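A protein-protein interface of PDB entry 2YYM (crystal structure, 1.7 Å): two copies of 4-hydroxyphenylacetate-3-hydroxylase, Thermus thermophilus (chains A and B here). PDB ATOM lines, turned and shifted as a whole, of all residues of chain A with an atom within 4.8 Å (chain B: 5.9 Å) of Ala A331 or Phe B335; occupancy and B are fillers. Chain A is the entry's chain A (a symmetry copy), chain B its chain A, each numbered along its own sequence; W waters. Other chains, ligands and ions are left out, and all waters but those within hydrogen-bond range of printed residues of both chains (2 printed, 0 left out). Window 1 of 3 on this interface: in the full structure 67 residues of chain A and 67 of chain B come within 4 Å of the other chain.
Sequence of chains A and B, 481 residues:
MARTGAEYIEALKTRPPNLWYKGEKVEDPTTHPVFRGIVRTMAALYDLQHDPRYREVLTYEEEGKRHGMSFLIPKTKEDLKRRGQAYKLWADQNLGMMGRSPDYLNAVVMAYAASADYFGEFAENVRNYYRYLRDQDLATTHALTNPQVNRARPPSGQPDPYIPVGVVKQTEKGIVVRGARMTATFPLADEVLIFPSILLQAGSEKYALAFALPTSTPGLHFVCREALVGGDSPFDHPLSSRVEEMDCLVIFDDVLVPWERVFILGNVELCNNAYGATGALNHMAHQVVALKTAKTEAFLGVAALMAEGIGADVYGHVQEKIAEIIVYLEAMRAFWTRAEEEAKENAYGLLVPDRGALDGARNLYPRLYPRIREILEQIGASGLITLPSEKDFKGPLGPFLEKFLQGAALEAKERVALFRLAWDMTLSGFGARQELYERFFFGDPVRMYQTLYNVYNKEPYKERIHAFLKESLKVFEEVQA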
ATOM      1  N   VAL A 327      -0.521  18.202  -5.758  1.00  0.00           N
ATOM      2  CA  VAL A 327       0.783  17.562  -5.879  1.00  0.00           C
ATOM      3  C   VAL A 327       1.030  17.198  -7.345  1.00  0.00           C
ATOM      4  O   VAL A 327       2.117  17.429  -7.878  1.00  0.00           O
ATOM      5  CB  VAL A 327       0.867  16.288  -5.005  1.00  0.00           C
ATOM      6  CG1 VAL A 327       2.117  15.473  -5.361  1.00  0.00           C
ATOM      7  CG2 VAL A 327       0.905  16.681  -3.523  1.00  0.00           C
ATOM      8  N   TYR A 328       0.015  16.649  -8.005  1.00  0.00           N
ATOM      9  CA  TYR A 328       0.167  16.263  -9.406  1.00  0.00           C
ATOM     10  C   TYR A 328       0.359  17.486 -10.294  1.00  0.00           C
ATOM     11  O   TYR A 328       1.119  17.447 -11.268  1.00  0.00           O
ATOM     12  CB  TYR A 328      -1.043  15.444  -9.873  1.00  0.00           C
ATOM     13  CG  TYR A 328      -1.277  14.194  -9.050  1.00  0.00           C
ATOM     14  CD1 TYR A 328      -0.219  13.557  -8.399  1.00  0.00           C
ATOM     15  CD2 TYR A 328      -2.549  13.638  -8.934  1.00  0.00           C
ATOM     16  CE1 TYR A 328      -0.425  12.401  -7.649  1.00  0.00           C
ATOM     17  CE2 TYR A 328      -2.766  12.477  -8.186  1.00  0.00           C
ATOM     18  CZ  TYR A 328      -1.694  11.868  -7.547  1.00  0.00           C
ATOM     19  OH  TYR A 328      -1.888  10.724  -6.802  1.00  0.00           O
ATOM     20  N   LEU A 329      -0.334  18.572  -9.965  1.00  0.00           N
ATOM     21  CA  LEU A 329      -0.187  19.808 -10.724  1.00  0.00           C
ATOM     22  C   LEU A 329       1.265  20.284 -10.618  1.00  0.00           C
ATOM     23  O   LEU A 329       1.896  20.625 -11.619  1.00  0.00           O
ATOM     24  CB  LEU A 329      -1.117  20.892 -10.169  1.00  0.00           C
ATOM     25  CG  LEU A 329      -0.904  22.295 -10.748  1.00  0.00           C
ATOM     26  CD1 LEU A 329      -1.066  22.254 -12.267  1.00  0.00           C
ATOM     27  CD2 LEU A 329      -1.903  23.267 -10.124  1.00  0.00           C
ATOM     28  N   GLU A 330       1.798  20.309  -9.401  1.00  0.00           N
ATOM     29  CA  GLU A 330       3.168  20.754  -9.217  1.00  0.00           C
ATOM     30  C   GLU A 330       4.155  19.830  -9.930  1.00  0.00           C
ATOM     31  O   GLU A 330       5.173  20.287 -10.450  1.00  0.00           O
ATOM     32  CB  GLU A 330       3.491  20.862  -7.726  1.00  0.00           C
ATOM     33  CG  GLU A 330       2.774  22.019  -7.025  1.00  0.00           C
ATOM     34  CD  GLU A 330       3.215  23.391  -7.533  1.00  0.00           C
ATOM     35  OE1 GLU A 330       4.390  23.535  -7.922  1.00  0.00           O
ATOM     36  OE2 GLU A 330       2.397  24.334  -7.524  1.00  0.00           O
ATOM     37  N   ALA A 331       3.857  18.536  -9.966  1.00  0.00           N
ATOM     38  CA  ALA A 331       4.738  17.590 -10.650  1.00  0.00           C
ATOM     39  C   ALA A 331       4.826  17.953 -12.135  1.00  0.00           C
ATOM     40  O   ALA A 331       5.909  17.964 -12.715  1.00  0.00           O
ATOM     41  CB  ALA A 331       4.213  16.160 -10.492  1.00  0.00           C
ATOM     42  N   MET A 332       3.688  18.261 -12.749  1.00  0.00           N
ATOM     43  CA  MET A 332       3.682  18.607 -14.170  1.00  0.00           C
ATOM     44  C   MET A 332       4.387  19.941 -14.422  1.00  0.00           C
ATOM     45  O   MET A 332       5.100  20.097 -15.413  1.00  0.00           O
ATOM     46  CB  MET A 332       2.244  18.645 -14.711  1.00  0.00           C
ATOM     47  CG  MET A 332       1.510  17.307 -14.622  1.00  0.00           C
ATOM     48  SD  MET A 332       2.473  15.917 -15.301  1.00  0.00           S
ATOM     49  CE  MET A 332       2.125  16.068 -17.018  1.00  0.00           C
ATOM     50  N   ARG A 333       4.190  20.905 -13.528  1.00  0.00           N
ATOM     51  CA  ARG A 333       4.855  22.196 -13.669  1.00  0.00           C
ATOM     52  C   ARG A 333       6.359  21.984 -13.579  1.00  0.00           C
ATOM     53  O   ARG A 333       7.130  22.620 -14.296  1.00  0.00           O
ATOM     54  CB  ARG A 333       4.421  23.153 -12.559  1.00  0.00           C
ATOM     55  CG  ARG A 333       3.066  23.768 -12.794  1.00  0.00           C
ATOM     56  CD  ARG A 333       2.641  24.628 -11.626  1.00  0.00           C
ATOM     57  NE  ARG A 333       1.384  25.311 -11.917  1.00  0.00           N
ATOM     58  CZ  ARG A 333       0.588  25.829 -10.992  1.00  0.00           C
ATOM     59  NH1 ARG A 333       0.916  25.744  -9.709  1.00  0.00           N
ATOM     60  NH2 ARG A 333      -0.538  26.428 -11.352  1.00  0.00           N
ATOM     61  N   ALA A 334       6.767  21.081 -12.692  1.00  0.00           N
ATOM     62  CA  ALA A 334       8.182  20.785 -12.504  1.00  0.00           C
ATOM     63  C   ALA A 334       8.801  20.168 -13.757  1.00  0.00           C
ATOM     64  O   ALA A 334       9.890  20.564 -14.171  1.00  0.00           O
ATOM     65  CB  ALA A 334       8.374  19.855 -11.303  1.00  0.00           C
ATOM     66  N   PHE A 335       8.113  19.200 -14.359  1.00  0.00           N
ATOM     67  CA  PHE A 335       8.630  18.565 -15.570  1.00  0.00           C
ATOM     68  C   PHE A 335       8.783  19.627 -16.657  1.00  0.00           C
ATOM     69  O   PHE A 335       9.797  19.680 -17.352  1.00  0.00           O
ATOM     70  CB  PHE A 335       7.673  17.476 -16.070  1.00  0.00           C
ATOM     71  CG  PHE A 335       7.787  16.163 -15.338  1.00  0.00           C
ATOM     72  CD1 PHE A 335       9.017  15.520 -15.215  1.00  0.00           C
ATOM     73  CD2 PHE A 335       6.653  15.543 -14.822  1.00  0.00           C
ATOM     74  CE1 PHE A 335       9.111  14.274 -14.594  1.00  0.00           C
ATOM     75  CE2 PHE A 335       6.737  14.298 -14.199  1.00  0.00           C
ATOM     76  CZ  PHE A 335       7.967  13.664 -14.085  1.00  0.00           C
ATOM     77  N   VAL B 289      15.021  16.924  -1.296  1.00  0.00           N
ATOM     78  CA  VAL B 289      14.817  16.559  -2.693  1.00  0.00           C
ATOM     79  C   VAL B 289      16.122  16.062  -3.322  1.00  0.00           C
ATOM     80  O   VAL B 289      16.112  15.110  -4.102  1.00  0.00           O
ATOM     81  CB  VAL B 289      14.198  17.732  -3.514  1.00  0.00           C
ATOM     82  CG1 VAL B 289      15.225  18.825  -3.768  1.00  0.00           C
ATOM     83  CG2 VAL B 289      13.622  17.198  -4.829  1.00  0.00           C
ATOM     84  N   GLU B 330      13.221  10.979 -12.637  1.00  0.00           N
ATOM     85  CA  GLU B 330      13.066  12.216 -13.383  1.00  0.00           C
ATOM     86  C   GLU B 330      12.102  13.173 -12.681  1.00  0.00           C
ATOM     87  O   GLU B 330      12.292  14.388 -12.719  1.00  0.00           O
ATOM     88  CB  GLU B 330      12.604  11.916 -14.810  1.00  0.00           C
ATOM     89  CG  GLU B 330      13.680  11.256 -15.676  1.00  0.00           C
ATOM     90  CD  GLU B 330      14.883  12.162 -15.929  1.00  0.00           C
ATOM     91  OE1 GLU B 330      14.702  13.392 -15.999  1.00  0.00           O
ATOM     92  OE2 GLU B 330      16.011  11.647 -16.080  1.00  0.00           O
ATOM     93  N   ALA B 331      11.076  12.633 -12.033  1.00  0.00           N
ATOM     94  CA  ALA B 331      10.123  13.479 -11.315  1.00  0.00           C
ATOM     95  C   ALA B 331      10.851  14.246 -10.207  1.00  0.00           C
ATOM     96  O   ALA B 331      10.640  15.444 -10.030  1.00  0.00           O
ATOM     97  CB  ALA B 331       9.001  12.629 -10.712  1.00  0.00           C
ATOM     98  N   MET B 332      11.716  13.559  -9.467  1.00  0.00           N
ATOM     99  CA  MET B 332      12.443  14.213  -8.379  1.00  0.00           C
ATOM    100  C   MET B 332      13.443  15.239  -8.915  1.00  0.00           C
ATOM    101  O   MET B 332      13.616  16.311  -8.333  1.00  0.00           O
ATOM    102  CB  MET B 332      13.156  13.170  -7.503  1.00  0.00           C
ATOM    103  CG  MET B 332      12.212  12.184  -6.816  1.00  0.00           C
ATOM    104  SD  MET B 332      10.834  13.001  -5.947  1.00  0.00           S
ATOM    105  CE  MET B 332      11.601  13.429  -4.423  1.00  0.00           C
ATOM    106  N   ARG B 333      14.103  14.917 -10.023  1.00  0.00           N
ATOM    107  CA  ARG B 333      15.046  15.853 -10.625  1.00  0.00           C
ATOM    108  C   ARG B 333      14.288  17.099 -11.060  1.00  0.00           C
ATOM    109  O   ARG B 333      14.784  18.217 -10.929  1.00  0.00           O
ATOM    110  CB  ARG B 333      15.721  15.230 -11.847  1.00  0.00           C
ATOM    111  CG  ARG B 333      16.824  14.266 -11.495  1.00  0.00           C
ATOM    112  CD  ARG B 333      17.394  13.606 -12.731  1.00  0.00           C
ATOM    113  NE  ARG B 333      18.537  12.767 -12.387  1.00  0.00           N
ATOM    114  CZ  ARG B 333      19.011  11.801 -13.163  1.00  0.00           C
ATOM    115  NH1 ARG B 333      18.438  11.548 -14.333  1.00  0.00           N
ATOM    116  NH2 ARG B 333      20.053  11.086 -12.764  1.00  0.00           N
ATOM    117  N   ALA B 334      13.080  16.893 -11.578  1.00  0.00           N
ATOM    118  CA  ALA B 334      12.252  18.002 -12.037  1.00  0.00           C
ATOM    119  C   ALA B 334      11.852  18.923 -10.885  1.00  0.00           C
ATOM    120  O   ALA B 334      11.931  20.145 -11.011  1.00  0.00           O
ATOM    121  CB  ALA B 334      11.005  17.472 -12.750  1.00  0.00           C
ATOM    122  N   PHE B 335      11.422  18.343  -9.767  1.00  0.00           N
ATOM    123  CA  PHE B 335      11.032  19.152  -8.614  1.00  0.00           C
ATOM    124  C   PHE B 335      12.236  19.971  -8.154  1.00  0.00           C
ATOM    125  O   PHE B 335      12.122  21.164  -7.876  1.00  0.00           O
ATOM    126  CB  PHE B 335      10.562  18.265  -7.454  1.00  0.00           C
ATOM    127  CG  PHE B 335       9.143  17.772  -7.584  1.00  0.00           C
ATOM    128  CD1 PHE B 335       8.094  18.665  -7.790  1.00  0.00           C
ATOM    129  CD2 PHE B 335       8.852  16.418  -7.441  1.00  0.00           C
ATOM    130  CE1 PHE B 335       6.775  18.214  -7.845  1.00  0.00           C
ATOM    131  CE2 PHE B 335       7.537  15.958  -7.495  1.00  0.00           C
ATOM    132  CZ  PHE B 335       6.498  16.857  -7.697  1.00  0.00           C
ATOM    133  N   TRP B 336      13.385  19.304  -8.073  1.00  0.00           N
ATOM    134  CA  TRP B 336      14.643  19.921  -7.656  1.00  0.00           C
ATOM    135  C   TRP B 336      14.967  21.122  -8.547  1.00  0.00           C
ATOM    136  O   TRP B 336      15.221  22.220  -8.060  1.00  0.00           O
ATOM    137  CB  TRP B 336      15.750  18.867  -7.747  1.00  0.00           C
ATOM    138  CG  TRP B 336      17.105  19.252  -7.228  1.00  0.00           C
ATOM    139  CD1 TRP B 336      17.528  20.485  -6.811  1.00  0.00           C
ATOM    140  CD2 TRP B 336      18.244  18.390  -7.148  1.00  0.00           C
ATOM    141  NE1 TRP B 336      18.869  20.439  -6.481  1.00  0.00           N
ATOM    142  CE2 TRP B 336      19.330  19.165  -6.681  1.00  0.00           C
ATOM    143  CE3 TRP B 336      18.453  17.034  -7.432  1.00  0.00           C
ATOM    144  CZ2 TRP B 336      20.610  18.625  -6.493  1.00  0.00           C
ATOM    145  CZ3 TRP B 336      19.724  16.497  -7.247  1.00  0.00           C
ATOM    146  CH2 TRP B 336      20.786  17.295  -6.782  1.00  0.00           C
ATOM    147  N   THR B 337      14.958  20.910  -9.858  1.00  0.00           N
ATOM    148  CA  THR B 337      15.235  21.989 -10.799  1.00  0.00           C
ATOM    149  C   THR B 337      14.269  23.161 -10.632  1.00  0.00           C
ATOM    150  O   THR B 337      14.696  24.309 -10.527  1.00  0.00           O
ATOM    151  CB  THR B 337      15.164  21.478 -12.250  1.00  0.00           C
ATOM    152  OG1 THR B 337      16.257  20.589 -12.483  1.00  0.00           O
ATOM    153  CG2 THR B 337      15.237  22.633 -13.246  1.00  0.00           C
ATOM    154  N   ARG B 338      12.969  22.887 -10.597  1.00  0.00           N
ATOM    155  CA  ARG B 338      12.009  23.977 -10.458  1.00  0.00           C
ATOM    156  C   ARG B 338      12.130  24.692  -9.115  1.00  0.00           C
ATOM    157  O   ARG B 338      11.901  25.897  -9.028  1.00  0.00           O
ATOM    158  CB  ARG B 338      10.575  23.474 -10.651  1.00  0.00           C
ATOM    159  CG  ARG B 338       9.541  24.589 -10.608  1.00  0.00           C
ATOM    160  CD  ARG B 338       8.148  24.085 -10.978  1.00  0.00           C
ATOM    161  NE  ARG B 338       7.122  25.091 -10.703  1.00  0.00           N
ATOM    162  CZ  ARG B 338       6.772  26.068 -11.533  1.00  0.00           C
ATOM    163  NH1 ARG B 338       7.361  26.187 -12.719  1.00  0.00           N
ATOM    164  NH2 ARG B 338       5.830  26.935 -11.175  1.00  0.00           N
ATOM    165  N   ALA B 339      12.487  23.952  -8.071  1.00  0.00           N
ATOM    166  CA  ALA B 339      12.628  24.550  -6.750  1.00  0.00           C
ATOM    167  C   ALA B 339      13.695  25.642  -6.776  1.00  0.00           C
ATOM    168  O   ALA B 339      13.538  26.691  -6.156  1.00  0.00           O
ATOM    169  CB  ALA B 339      12.994  23.482  -5.725  1.00  0.00           C
ATOM    170  N   GLU B 340      14.773  25.403  -7.513  1.00  0.00           N
ATOM    171  CA  GLU B 340      15.856  26.376  -7.599  1.00  0.00           C
ATOM    172  C   GLU B 340      15.570  27.485  -8.608  1.00  0.00           C
ATOM    173  O   GLU B 340      15.817  28.659  -8.334  1.00  0.00           O
ATOM    174  CB  GLU B 340      17.167  25.671  -7.962  1.00  0.00           C
ATOM    175  CG  GLU B 340      17.580  24.609  -6.954  1.00  0.00           C
ATOM    176  CD  GLU B 340      18.848  23.876  -7.337  1.00  0.00           C
ATOM    177  OE1 GLU B 340      19.189  23.862  -8.538  1.00  0.00           O
ATOM    178  OE2 GLU B 340      19.493  23.294  -6.440  1.00  0.00           O
ATOM    179  N   GLY B 356       6.108  25.472  -3.840  1.00  0.00           N
ATOM    180  CA  GLY B 356       5.226  24.633  -4.637  1.00  0.00           C
ATOM    181  C   GLY B 356       5.919  23.360  -5.094  1.00  0.00           C
ATOM    182  O   GLY B 356       5.389  22.257  -4.939  1.00  0.00           O
ATOM    183  N   ALA B 357       7.119  23.508  -5.649  1.00  0.00           N
ATOM    184  CA  ALA B 357       7.883  22.366  -6.133  1.00  0.00           C
ATOM    185  C   ALA B 357       8.334  21.447  -5.001  1.00  0.00           C
ATOM    186  O   ALA B 357       8.306  20.223  -5.141  1.00  0.00           O
ATOM    187  CB  ALA B 357       9.097  22.853  -6.923  1.00  0.00           C
ATOM    188  N   LEU B 358       8.740  22.029  -3.877  1.00  0.00           N
ATOM    189  CA  LEU B 358       9.203  21.222  -2.753  1.00  0.00           C
ATOM    190  C   LEU B 358       8.054  20.533  -2.018  1.00  0.00           C
ATOM    191  O   LEU B 358       8.224  19.428  -1.503  1.00  0.00           O
ATOM    192  CB  LEU B 358      10.041  22.085  -1.799  1.00  0.00           C
ATOM    193  CG  LEU B 358      11.340  22.582  -2.462  1.00  0.00           C
ATOM    194  CD1 LEU B 358      12.100  23.505  -1.532  1.00  0.00           C
ATOM    195  CD2 LEU B 358      12.203  21.391  -2.846  1.00  0.00           C
ATOM    196  N   GLY B 360       5.499  19.544  -3.507  1.00  0.00           N
ATOM    197  CA  GLY B 360       5.176  18.463  -4.418  1.00  0.00           C
ATOM    198  C   GLY B 360       6.109  17.285  -4.187  1.00  0.00           C
ATOM    199  O   GLY B 360       5.662  16.146  -4.067  1.00  0.00           O
ATOM    200  N   ALA B 361       7.409  17.560  -4.106  1.00  0.00           N
ATOM    201  CA  ALA B 361       8.404  16.508  -3.906  1.00  0.00           C
ATOM    202  C   ALA B 361       8.281  15.761  -2.579  1.00  0.00           C
ATOM    203  O   ALA B 361       8.331  14.529  -2.545  1.00  0.00           O
ATOM    204  CB  ALA B 361       9.817  17.097  -4.030  1.00  0.00           C
ATOM    205  N   LEU B 364       5.024  13.733  -2.561  1.00  0.00           N
ATOM    206  CA  LEU B 364       4.925  12.680  -3.558  1.00  0.00           C
ATOM    207  C   LEU B 364       5.879  11.523  -3.257  1.00  0.00           C
ATOM    208  O   LEU B 364       5.495  10.361  -3.372  1.00  0.00           O
ATOM    209  CB  LEU B 364       5.216  13.215  -4.967  1.00  0.00           C
ATOM    210  CG  LEU B 364       5.043  12.179  -6.090  1.00  0.00           C
ATOM    211  CD1 LEU B 364       3.594  11.705  -6.130  1.00  0.00           C
ATOM    212  CD2 LEU B 364       5.439  12.779  -7.432  1.00  0.00           C
HETATM  213  O   HOH W   1       5.677  25.826  -8.334  1.00  0.00           O
HETATM  214  O   HOH W   2       6.449  22.229  -9.026  1.00  0.00           O
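The side-chain carboxylate (OE1) of Glu A330 lies close to the backbone carbonyl oxygen (O) of Gly B356 (3.4 Å).
NH1 of Arg B333 is in salt-bridge range of OE2 of Glu B330, 3.0 Å away. The guanidinium group (NH1) of Arg A333 is in salt-bridge range of the side-chain carboxylate (OE2) of Glu A330.
Among the printed residues, merely in contact across the chains: Val A327 with Gly B360, Val A327 with Leu B364, Glu A330 with Phe B335, Glu A330 with Ala B357, Ala A331 with Phe B335, Arg A333 with Arg B338, Ala A334 with Ala B334, Ala A334 with Phe B335, Ala A334 with Arg B338, Phe A335 with Glu B330, Phe A335 with Ala B331 and Phe A335 with Ala B334.
Ala A331 touches one residue of chain B. Of the printed residues of chain A, Phe B335 touches Glu A330, Ala A331 and Ala A334. Printed residues of chain A within 4 Å of Glu B330: Phe A335 (3.7 Å). Of the printed residues of chain A, Arg B338 touches Arg A333 (3.8 Å) and Ala A334 (3.6 Å). Of the printed residues of chain A, Ala B334 touches Ala A334 and Phe A335. Leu A329 touches none of the printed residues of chain B. Val B289 touches none of the printed residues of chain A. The nearest residue of chain A that does not touch Phe B335 is Val A327 (4.4 Å). The nearest printed residue of chain A that does not touch Ala B331 is Ala A334 (5.1 Å).
Of the 9 printed residues of chain A, 6 touch a printed residue of chain B. Among the printed residues, 13 pairs touch across the chains. Among the printed residues, no Asp or Glu carboxylate lies within 4 Å of a Lys or Arg side-chain nitrogen of the other chain.
Glu A330 touches Phe B335, and with the chains exchanged Phe A335 touches Glu B330. Ala A331 touches Phe B335, and with the chains exchanged Phe A335 touches Ala B331. Ala B334 touches its own counterpart, Ala A334. Ala A334 touches Phe B335, and with the chains exchanged Phe A335 touches Ala B334. Positions printed for both chains: 330, 331, 332, 333, 334 and 335.
Water W1 bridges the side-chain carboxylate (OE1) of Glu A330 (2.7 Å) and the guanidinium group (NE) of Arg B338 (2.9 Å). Water W2 lies within hydrogen-bond range of the side-chain carboxylate of Glu A330 (2.7 Å) and the guanidinium group of Arg B338 (3.4 Å).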
